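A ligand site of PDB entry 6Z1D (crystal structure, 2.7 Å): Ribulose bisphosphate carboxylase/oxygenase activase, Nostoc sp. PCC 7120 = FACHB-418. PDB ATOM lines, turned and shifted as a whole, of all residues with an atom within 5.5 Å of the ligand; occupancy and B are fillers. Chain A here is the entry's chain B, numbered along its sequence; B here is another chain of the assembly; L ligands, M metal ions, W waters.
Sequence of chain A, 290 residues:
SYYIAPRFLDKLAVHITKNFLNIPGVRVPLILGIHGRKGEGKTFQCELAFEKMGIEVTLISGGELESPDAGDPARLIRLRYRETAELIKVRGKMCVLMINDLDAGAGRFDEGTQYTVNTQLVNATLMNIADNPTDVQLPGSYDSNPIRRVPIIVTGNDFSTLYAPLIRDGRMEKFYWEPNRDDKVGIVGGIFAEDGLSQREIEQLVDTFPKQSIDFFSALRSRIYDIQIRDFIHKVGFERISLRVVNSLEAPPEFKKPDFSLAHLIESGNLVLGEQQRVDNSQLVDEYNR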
ATOM      1  N   TYR A   2      -4.471  11.789 -39.227  1.00  0.00           N
ATOM      2  CA  TYR A   2      -3.731  11.331 -38.059  1.00  0.00           C
ATOM      3  C   TYR A   2      -2.278  11.031 -38.398  1.00  0.00           C
ATOM      4  O   TYR A   2      -1.944  10.684 -39.530  1.00  0.00           O
ATOM      5  CB  TYR A   2      -4.435  10.133 -37.407  1.00  0.00           C
ATOM      6  CG  TYR A   2      -5.825  10.503 -36.949  1.00  0.00           C
ATOM      7  CD1 TYR A   2      -6.042  11.664 -36.216  1.00  0.00           C
ATOM      8  CD2 TYR A   2      -6.933   9.724 -37.285  1.00  0.00           C
ATOM      9  CE1 TYR A   2      -7.308  12.026 -35.800  1.00  0.00           C
ATOM     10  CE2 TYR A   2      -8.213  10.088 -36.872  1.00  0.00           C
ATOM     11  CZ  TYR A   2      -8.389  11.243 -36.130  1.00  0.00           C
ATOM     12  OH  TYR A   2      -9.643  11.620 -35.726  1.00  0.00           O
ATOM     13  N   TYR A   3      -1.419  11.171 -37.385  1.00  0.00           N
ATOM     14  CA  TYR A   3       0.030  11.167 -37.530  1.00  0.00           C
ATOM     15  C   TYR A   3       0.666   9.987 -36.836  1.00  0.00           C
ATOM     16  O   TYR A   3       0.486   9.803 -35.636  1.00  0.00           O
ATOM     17  CB  TYR A   3       0.584  12.435 -36.910  1.00  0.00           C
ATOM     18  CG  TYR A   3       2.089  12.507 -36.792  1.00  0.00           C
ATOM     19  CD1 TYR A   3       2.874  12.957 -37.845  1.00  0.00           C
ATOM     20  CD2 TYR A   3       2.724  12.170 -35.607  1.00  0.00           C
ATOM     21  CE1 TYR A   3       4.241  13.036 -37.726  1.00  0.00           C
ATOM     22  CE2 TYR A   3       4.095  12.249 -35.474  1.00  0.00           C
ATOM     23  CZ  TYR A   3       4.843  12.681 -36.538  1.00  0.00           C
ATOM     24  OH  TYR A   3       6.215  12.760 -36.405  1.00  0.00           O
ATOM     25  N   ILE A   4       1.418   9.190 -37.589  1.00  0.00           N
ATOM     26  CA  ILE A   4       2.131   8.042 -37.034  1.00  0.00           C
ATOM     27  C   ILE A   4       3.585   8.457 -36.789  1.00  0.00           C
ATOM     28  O   ILE A   4       4.245   8.983 -37.691  1.00  0.00           O
ATOM     29  CB  ILE A   4       2.023   6.794 -37.969  1.00  0.00           C
ATOM     30  CG1 ILE A   4       2.850   5.627 -37.452  1.00  0.00           C
ATOM     31  CG2 ILE A   4       2.475   7.111 -39.384  1.00  0.00           C
ATOM     32  CD1 ILE A   4       2.319   5.010 -36.210  1.00  0.00           C
ATOM     33  N   ARG A  37       3.135   3.794 -20.760  1.00  0.00           N
ATOM     34  CA  ARG A  37       1.998   4.353 -20.050  1.00  0.00           C
ATOM     35  C   ARG A  37       0.734   4.189 -20.881  1.00  0.00           C
ATOM     36  O   ARG A  37       0.792   4.159 -22.109  1.00  0.00           O
ATOM     37  CB  ARG A  37       2.213   5.829 -19.703  1.00  0.00           C
ATOM     38  CG  ARG A  37       1.002   6.483 -19.030  1.00  0.00           C
ATOM     39  CD  ARG A  37       1.289   7.888 -18.548  1.00  0.00           C
ATOM     40  NE  ARG A  37       1.696   8.780 -19.630  1.00  0.00           N
ATOM     41  CZ  ARG A  37       2.113  10.028 -19.441  1.00  0.00           C
ATOM     42  NH1 ARG A  37       2.179  10.539 -18.209  1.00  0.00           N
ATOM     43  NH2 ARG A  37       2.472  10.772 -20.479  1.00  0.00           N
ATOM     44  N   LYS A  38      -0.399   4.056 -20.204  1.00  0.00           N
ATOM     45  CA  LYS A  38      -1.678   3.859 -20.880  1.00  0.00           C
ATOM     46  C   LYS A  38      -2.102   5.122 -21.632  1.00  0.00           C
ATOM     47  O   LYS A  38      -1.866   6.240 -21.177  1.00  0.00           O
ATOM     48  CB  LYS A  38      -2.728   3.455 -19.850  1.00  0.00           C
ATOM     49  CG  LYS A  38      -4.144   3.284 -20.346  1.00  0.00           C
ATOM     50  CD  LYS A  38      -5.073   3.080 -19.154  1.00  0.00           C
ATOM     51  CE  LYS A  38      -6.539   3.240 -19.531  1.00  0.00           C
ATOM     52  NZ  LYS A  38      -6.998   2.154 -20.435  1.00  0.00           N
ATOM     53  N   GLY A  39      -2.736   4.918 -22.786  1.00  0.00           N
ATOM     54  CA  GLY A  39      -3.293   6.011 -23.556  1.00  0.00           C
ATOM     55  C   GLY A  39      -2.255   6.855 -24.274  1.00  0.00           C
ATOM     56  O   GLY A  39      -2.439   8.063 -24.396  1.00  0.00           O
ATOM     57  N   GLU A  40      -1.182   6.234 -24.751  1.00  0.00           N
ATOM     58  CA  GLU A  40      -0.146   6.942 -25.502  1.00  0.00           C
ATOM     59  C   GLU A  40      -0.154   6.558 -26.965  1.00  0.00           C
ATOM     60  O   GLU A  40       0.807   6.823 -27.685  1.00  0.00           O
ATOM     61  CB  GLU A  40       1.247   6.661 -24.918  1.00  0.00           C
ATOM     62  CG  GLU A  40       1.433   7.037 -23.468  1.00  0.00           C
ATOM     63  CD  GLU A  40       1.623   8.524 -23.240  1.00  0.00           C
ATOM     64  OE1 GLU A  40       1.152   9.345 -24.061  1.00  0.00           O
ATOM     65  OE2 GLU A  40       2.251   8.877 -22.215  1.00  0.00           O
ATOM     66  N   GLY A  41      -1.231   5.935 -27.428  1.00  0.00           N
ATOM     67  CA  GLY A  41      -1.400   5.635 -28.840  1.00  0.00           C
ATOM     68  C   GLY A  41      -0.710   4.365 -29.327  1.00  0.00           C
ATOM     69  O   GLY A  41      -0.495   4.193 -30.521  1.00  0.00           O
ATOM     70  N   LYS A  42      -0.371   3.470 -28.407  1.00  0.00           N
ATOM     71  CA  LYS A  42       0.147   2.155 -28.789  1.00  0.00           C
ATOM     72  C   LYS A  42      -0.804   1.464 -29.755  1.00  0.00           C
ATOM     73  O   LYS A  42      -0.408   1.082 -30.855  1.00  0.00           O
ATOM     74  CB  LYS A  42       0.365   1.289 -27.554  1.00  0.00           C
ATOM     75  CG  LYS A  42       1.646   1.601 -26.822  1.00  0.00           C
ATOM     76  CD  LYS A  42       1.751   0.820 -25.521  1.00  0.00           C
ATOM     77  CE  LYS A  42       1.216   1.597 -24.326  1.00  0.00           C
ATOM     78  NZ  LYS A  42      -0.064   1.075 -23.798  1.00  0.00           N
ATOM     79  N   THR A  43      -2.061   1.309 -29.365  1.00  0.00           N
ATOM     80  CA  THR A  43      -3.030   0.662 -30.251  1.00  0.00           C
ATOM     81  C   THR A  43      -3.315   1.508 -31.494  1.00  0.00           C
ATOM     82  O   THR A  43      -3.286   1.011 -32.608  1.00  0.00           O
ATOM     83  CB  THR A  43      -4.368   0.390 -29.546  1.00  0.00           C
ATOM     84  OG1 THR A  43      -4.151  -0.517 -28.466  1.00  0.00           O
ATOM     85  CG2 THR A  43      -5.380  -0.204 -30.509  1.00  0.00           C
ATOM     86  N   PHE A  44      -3.602   2.789 -31.292  1.00  0.00           N
ATOM     87  CA  PHE A  44      -4.011   3.639 -32.389  1.00  0.00           C
ATOM     88  C   PHE A  44      -2.949   3.703 -33.494  1.00  0.00           C
ATOM     89  O   PHE A  44      -3.264   3.622 -34.677  1.00  0.00           O
ATOM     90  CB  PHE A  44      -4.321   5.035 -31.877  1.00  0.00           C
ATOM     91  CG  PHE A  44      -5.123   5.851 -32.818  1.00  0.00           C
ATOM     92  CD1 PHE A  44      -4.506   6.592 -33.809  1.00  0.00           C
ATOM     93  CD2 PHE A  44      -6.500   5.895 -32.714  1.00  0.00           C
ATOM     94  CE1 PHE A  44      -5.242   7.351 -34.680  1.00  0.00           C
ATOM     95  CE2 PHE A  44      -7.251   6.657 -33.588  1.00  0.00           C
ATOM     96  CZ  PHE A  44      -6.628   7.386 -34.572  1.00  0.00           C
ATOM     97  N   GLN A  45      -1.692   3.835 -33.101  1.00  0.00           N
ATOM     98  CA  GLN A  45      -0.612   3.918 -34.071  1.00  0.00           C
ATOM     99  C   GLN A  45      -0.329   2.595 -34.762  1.00  0.00           C
ATOM    100  O   GLN A  45       0.113   2.576 -35.911  1.00  0.00           O
ATOM    101  CB  GLN A  45       0.640   4.435 -33.396  1.00  0.00           C
ATOM    102  CG  GLN A  45       0.575   5.900 -33.073  1.00  0.00           C
ATOM    103  CD  GLN A  45       1.871   6.395 -32.517  1.00  0.00           C
ATOM    104  OE1 GLN A  45       2.549   7.234 -33.113  1.00  0.00           O
ATOM    105  NE2 GLN A  45       2.249   5.857 -31.367  1.00  0.00           N
ATOM    106  N   LEU A  48      -2.871   2.689 -37.432  1.00  0.00           N
ATOM    107  CA  LEU A  48      -2.411   3.581 -38.486  1.00  0.00           C
ATOM    108  C   LEU A  48      -1.391   2.877 -39.384  1.00  0.00           C
ATOM    109  O   LEU A  48      -1.520   2.890 -40.603  1.00  0.00           O
ATOM    110  CB  LEU A  48      -1.809   4.858 -37.883  1.00  0.00           C
ATOM    111  CG  LEU A  48      -2.824   5.817 -37.241  1.00  0.00           C
ATOM    112  CD1 LEU A  48      -2.114   7.006 -36.612  1.00  0.00           C
ATOM    113  CD2 LEU A  48      -3.875   6.289 -38.237  1.00  0.00           C
ATOM    114  N   ASN A 100      -4.333  -6.781 -27.639  1.00  0.00           N
ATOM    115  CA  ASN A 100      -4.425  -5.442 -27.088  1.00  0.00           C
ATOM    116  C   ASN A 100      -4.599  -5.410 -25.582  1.00  0.00           C
ATOM    117  O   ASN A 100      -5.318  -6.246 -25.032  1.00  0.00           O
ATOM    118  CB  ASN A 100      -5.631  -4.763 -27.709  1.00  0.00           C
ATOM    119  CG  ASN A 100      -5.277  -3.582 -28.542  1.00  0.00           C
ATOM    120  OD1 ASN A 100      -4.164  -3.055 -28.447  1.00  0.00           O
ATOM    121  ND2 ASN A 100      -6.210  -3.148 -29.360  1.00  0.00           N
ATOM    122  N   ASP A 101      -3.972  -4.441 -24.926  1.00  0.00           N
ATOM    123  CA  ASP A 101      -4.200  -4.175 -23.513  1.00  0.00           C
ATOM    124  C   ASP A 101      -3.999  -5.418 -22.656  1.00  0.00           C
ATOM    125  O   ASP A 101      -4.908  -5.847 -21.935  1.00  0.00           O
ATOM    126  CB  ASP A 101      -5.625  -3.654 -23.287  1.00  0.00           C
ATOM    127  CG  ASP A 101      -5.943  -2.446 -24.126  1.00  0.00           C
ATOM    128  OD1 ASP A 101      -5.000  -1.723 -24.524  1.00  0.00           O
ATOM    129  OD2 ASP A 101      -7.138  -2.209 -24.395  1.00  0.00           O
ATOM    130  N   THR A 155       0.330  -5.416 -27.025  1.00  0.00           N
ATOM    131  CA  THR A 155       0.432  -4.163 -26.268  1.00  0.00           C
ATOM    132  C   THR A 155      -0.003  -4.345 -24.817  1.00  0.00           C
ATOM    133  O   THR A 155      -0.822  -5.208 -24.501  1.00  0.00           O
ATOM    134  CB  THR A 155      -0.408  -3.012 -26.869  1.00  0.00           C
ATOM    135  OG1 THR A 155      -1.802  -3.321 -26.749  1.00  0.00           O
ATOM    136  CG2 THR A 155      -0.025  -2.736 -28.327  1.00  0.00           C
ATOM    137  N   TRP A 177       7.305   2.474 -25.514  1.00  0.00           N
ATOM    138  CA  TRP A 177       6.717   3.621 -26.178  1.00  0.00           C
ATOM    139  C   TRP A 177       6.377   4.762 -25.216  1.00  0.00           C
ATOM    140  O   TRP A 177       5.459   4.657 -24.404  1.00  0.00           O
ATOM    141  CB  TRP A 177       5.475   3.198 -26.987  1.00  0.00           C
ATOM    142  CG  TRP A 177       4.812   4.375 -27.619  1.00  0.00           C
ATOM    143  CD1 TRP A 177       3.556   4.852 -27.359  1.00  0.00           C
ATOM    144  CD2 TRP A 177       5.377   5.259 -28.589  1.00  0.00           C
ATOM    145  NE1 TRP A 177       3.304   5.958 -28.120  1.00  0.00           N
ATOM    146  CE2 TRP A 177       4.415   6.239 -28.883  1.00  0.00           C
ATOM    147  CE3 TRP A 177       6.619   5.320 -29.240  1.00  0.00           C
ATOM    148  CZ2 TRP A 177       4.629   7.263 -29.798  1.00  0.00           C
ATOM    149  CZ3 TRP A 177       6.831   6.339 -30.147  1.00  0.00           C
ATOM    150  CH2 TRP A 177       5.848   7.294 -30.427  1.00  0.00           C
ATOM    151  N   ILE A 187       1.265  14.141 -33.345  1.00  0.00           N
ATOM    152  CA  ILE A 187       0.018  13.449 -33.002  1.00  0.00           C
ATOM    153  C   ILE A 187      -1.063  14.431 -32.555  1.00  0.00           C
ATOM    154  O   ILE A 187      -2.201  14.336 -33.012  1.00  0.00           O
ATOM    155  CB  ILE A 187       0.243  12.381 -31.882  1.00  0.00           C
ATOM    156  CG1 ILE A 187       1.170  11.271 -32.363  1.00  0.00           C
ATOM    157  CG2 ILE A 187      -1.094  11.775 -31.407  1.00  0.00           C
ATOM    158  CD1 ILE A 187       1.855  10.514 -31.243  1.00  0.00           C
ATOM    159  N   GLY A 190      -2.425  16.371 -35.414  1.00  0.00           N
ATOM    160  CA  GLY A 190      -3.409  15.609 -36.158  1.00  0.00           C
ATOM    161  C   GLY A 190      -4.753  15.518 -35.456  1.00  0.00           C
ATOM    162  O   GLY A 190      -5.791  15.482 -36.113  1.00  0.00           O
ATOM    163  N   ILE A 191      -4.734  15.464 -34.125  1.00  0.00           N
ATOM    164  CA  ILE A 191      -5.972  15.411 -33.348  1.00  0.00           C
ATOM    165  C   ILE A 191      -6.790  16.674 -33.580  1.00  0.00           C
ATOM    166  O   ILE A 191      -8.017  16.623 -33.621  1.00  0.00           O
ATOM    167  CB  ILE A 191      -5.699  15.248 -31.831  1.00  0.00           C
ATOM    168  CG1 ILE A 191      -5.188  13.838 -31.544  1.00  0.00           C
ATOM    169  CG2 ILE A 191      -6.970  15.496 -31.007  1.00  0.00           C
ATOM    170  CD1 ILE A 191      -4.595  13.686 -30.156  1.00  0.00           C
ATOM    171  N   ILE A 214      -1.196  11.250 -24.669  1.00  0.00           N
ATOM    172  CA  ILE A 214      -1.904  11.641 -25.890  1.00  0.00           C
ATOM    173  C   ILE A 214      -3.426  11.616 -25.653  1.00  0.00           C
ATOM    174  O   ILE A 214      -4.160  12.447 -26.184  1.00  0.00           O
ATOM    175  CB  ILE A 214      -1.493  10.729 -27.092  1.00  0.00           C
ATOM    176  CG1 ILE A 214      -0.249  11.290 -27.773  1.00  0.00           C
ATOM    177  CG2 ILE A 214      -2.597  10.648 -28.151  1.00  0.00           C
ATOM    178  CD1 ILE A 214       0.905  11.581 -26.864  1.00  0.00           C
ATOM    179  N   ASP A 215      -3.869  10.676 -24.812  1.00  0.00           N
ATOM    180  CA  ASP A 215      -5.285  10.497 -24.479  1.00  0.00           C
ATOM    181  C   ASP A 215      -5.905  11.761 -23.882  1.00  0.00           C
ATOM    182  O   ASP A 215      -7.052  12.112 -24.178  1.00  0.00           O
ATOM    183  CB  ASP A 215      -5.438   9.361 -23.469  1.00  0.00           C
ATOM    184  CG  ASP A 215      -6.871   8.878 -23.331  1.00  0.00           C
ATOM    185  OD1 ASP A 215      -7.611   8.874 -24.350  1.00  0.00           O
ATOM    186  OD2 ASP A 215      -7.269   8.503 -22.208  1.00  0.00           O
ATOM    187  N   SER A 218      -6.876  14.193 -26.798  1.00  0.00           N
ATOM    188  CA  SER A 218      -8.086  13.908 -27.577  1.00  0.00           C
ATOM    189  C   SER A 218      -9.306  14.038 -26.677  1.00  0.00           C
ATOM    190  O   SER A 218     -10.413  14.340 -27.156  1.00  0.00           O
ATOM    191  CB  SER A 218      -8.023  12.524 -28.222  1.00  0.00           C
ATOM    192  OG  SER A 218      -7.831  11.513 -27.257  1.00  0.00           O
ATOM    193  N   ILE B 167     -14.627   2.299 -25.774  1.00  0.00           N
ATOM    194  CA  ILE B 167     -14.068   3.601 -25.396  1.00  0.00           C
ATOM    195  C   ILE B 167     -13.145   4.099 -26.490  1.00  0.00           C
ATOM    196  O   ILE B 167     -13.257   5.233 -26.933  1.00  0.00           O
ATOM    197  CB  ILE B 167     -13.299   3.509 -24.055  1.00  0.00           C
ATOM    198  CG1 ILE B 167     -14.244   3.109 -22.933  1.00  0.00           C
ATOM    199  CG2 ILE B 167     -12.630   4.841 -23.699  1.00  0.00           C
ATOM    200  CD1 ILE B 167     -13.578   2.365 -21.822  1.00  0.00           C
ATOM    201  N   ARG B 168     -12.241   3.229 -26.933  1.00  0.00           N
ATOM    202  CA  ARG B 168     -11.259   3.586 -27.938  1.00  0.00           C
ATOM    203  C   ARG B 168     -11.934   4.204 -29.185  1.00  0.00           C
ATOM    204  O   ARG B 168     -11.390   5.130 -29.791  1.00  0.00           O
ATOM    205  CB  ARG B 168     -10.443   2.348 -28.311  1.00  0.00           C
ATOM    206  CG  ARG B 168      -9.176   2.645 -29.045  1.00  0.00           C
ATOM    207  CD  ARG B 168      -8.250   1.446 -29.091  1.00  0.00           C
ATOM    208  NE  ARG B 168      -7.318   1.421 -27.963  1.00  0.00           N
ATOM    209  CZ  ARG B 168      -7.344   0.554 -26.951  1.00  0.00           C
ATOM    210  NH1 ARG B 168      -8.264  -0.415 -26.904  1.00  0.00           N
ATOM    211  NH2 ARG B 168      -6.450   0.644 -25.994  1.00  0.00           N
HETATM  212  P1  LIG L   1      -2.710   2.869 -25.579  1.00  0.00           P
HETATM  213  O1  LIG L   1      -2.874   1.811 -26.657  1.00  0.00           O
HETATM  214  O2  LIG L   1      -3.503   2.618 -24.305  1.00  0.00           O
HETATM  215  O3  LIG L   1      -1.261   3.251 -25.332  1.00  0.00           O
HETATM  216  P2  LIG L   1      -4.611   4.157 -27.290  1.00  0.00           P
HETATM  217  O4  LIG L   1      -5.843   3.574 -26.642  1.00  0.00           O
HETATM  218  O5  LIG L   1      -4.109   3.582 -28.592  1.00  0.00           O
HETATM  219  O6  LIG L   1      -3.401   4.178 -26.213  1.00  0.00           O
HETATM  220  O7  LIG L   1      -4.842   5.734 -27.497  1.00  0.00           O
HETATM  221  C1  LIG L   1      -5.631   6.518 -26.583  1.00  0.00           C
HETATM  222  C2  LIG L   1      -6.454   7.568 -27.322  1.00  0.00           C
HETATM  223  O8  LIG L   1      -5.644   8.659 -27.746  1.00  0.00           O
HETATM  224  C3  LIG L   1      -7.199   7.046 -28.549  1.00  0.00           C
HETATM  225  O9  LIG L   1      -8.532   6.683 -28.193  1.00  0.00           O
HETATM  226  C4  LIG L   1      -7.151   8.199 -29.531  1.00  0.00           C
HETATM  227  O10 LIG L   1      -8.363   8.970 -29.481  1.00  0.00           O
HETATM  228  C5  LIG L   1      -5.987   9.055 -29.075  1.00  0.00           C
HETATM  229  N1  LIG L   1      -4.817   8.795 -29.947  1.00  0.00           N
HETATM  230  C6  LIG L   1      -3.781   7.979 -29.667  1.00  0.00           C
HETATM  231  N2  LIG L   1      -2.892   7.974 -30.683  1.00  0.00           N
HETATM  232  C7  LIG L   1      -3.343   8.806 -31.622  1.00  0.00           C
HETATM  233  C8  LIG L   1      -2.878   9.256 -32.957  1.00  0.00           C
HETATM  234  N3  LIG L   1      -1.715   8.811 -33.485  1.00  0.00           N
HETATM  235  N4  LIG L   1      -3.666  10.131 -33.620  1.00  0.00           N
HETATM  236  C9  LIG L   1      -4.817  10.591 -33.104  1.00  0.00           C
HETATM  237  N5  LIG L   1      -5.295  10.214 -31.909  1.00  0.00           N
HETATM  238  C10 LIG L   1      -4.616   9.343 -31.142  1.00  0.00           C
HETATM  239 GD    GD M   1      -6.082   3.544 -23.441  1.00  0.00          GD
HETATM  240  O   HOH W   1      -2.559  12.444 -35.202  1.00  0.00           O
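Merely in contact with the ligand: Ile 214, Asp 215, Ile 187, Tyr 2, Ile 191, Leu 48, Gln 45, Lys 38 and Arg 37. Hydrophobic or aromatic side chains that line the ligand: Tyr 2, Phe 44, Leu 48, Ile 187, Ile 191 and Ile 214. Of the 25 residues printed, 18 come within 4 Å of the ligand. The nearest printed residue that does not touch the ligand is Asp 101 (4.6 Å).
Water W1 lies within hydrogen-bond range of the backbone NH of Tyr 3 (2.8 Å), the backbone carbonyl oxygen of Ile 187 (2.9 Å) and a nitrogen (N4) of the ligand (3.0 Å).
The backbone NH (N) of Glu 40 lies within hydrogen-bond range of an oxygen (O3) of the ligand (3.0 Å). O6 of the ligand is in hydrogen-bond range of N of Gly 41, 3.0 Å away. The backbone NH (N) of Lys 42 lies close to an oxygen (O3) of the ligand (3.2 Å). The side-chain hydroxyl (OG) of Ser 218 lies within hydrogen-bond range of an oxygen (O10) of the ligand (3.4 Å). N of Thr 43 lies within hydrogen-bond range of O1 of the ligand, 2.9 Å away. The backbone carbonyl oxygen of Tyr 3 is in hydrogen-bond range of a nitrogen (N3) of the ligand (3.2 Å). The backbone NH (N) of Phe 44 is in hydrogen-bond range of an oxygen (O5) of the ligand. An oxygen (O1) of the ligand lies within hydrogen-bond range of the side-chain hydroxyl of Thr 43 (3.2 Å). NE of Arg 168 of chain B lies within salt-bridge range of O4 of the ligand. The side-chain amino group of Lys 42 lies within salt-bridge range of an oxygen (O3) of the ligand. N of Gly 39 is in hydrogen-bond range of O2 of the ligand (2.9 Å).
The backbone carbonyl oxygen (O) of Gly 39 sits at hydrogen-bond distance from the backbone NH (N) of Asp 215 (3.0 Å). The backbone NH (N) of Ile 214 sits at hydrogen-bond distance from the backbone carbonyl oxygen (O) of Gly 39, at 3.4 Å. NH2 of Arg 37 lies within salt-bridge range of OE2 of Glu 40 (2.6 Å). NE1 of Trp 177 sits close to NE2 of Gln 45, at 3.4 Å. The side-chain hydroxyl (OG1) of Thr 43 sits at hydrogen-bond distance from the side-chain amide oxygen (OD1) of Asn 100 (2.5 Å). The backbone carbonyl oxygen (O) of Gly 41 lies close to the side-chain amide nitrogen (NE2) of Gln 45 (3.3 Å). OE1 of Glu 40 sits at hydrogen-bond distance from N of Ile 214. NE1 of Trp 177 lies within hydrogen-bond range of O of Glu 40.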
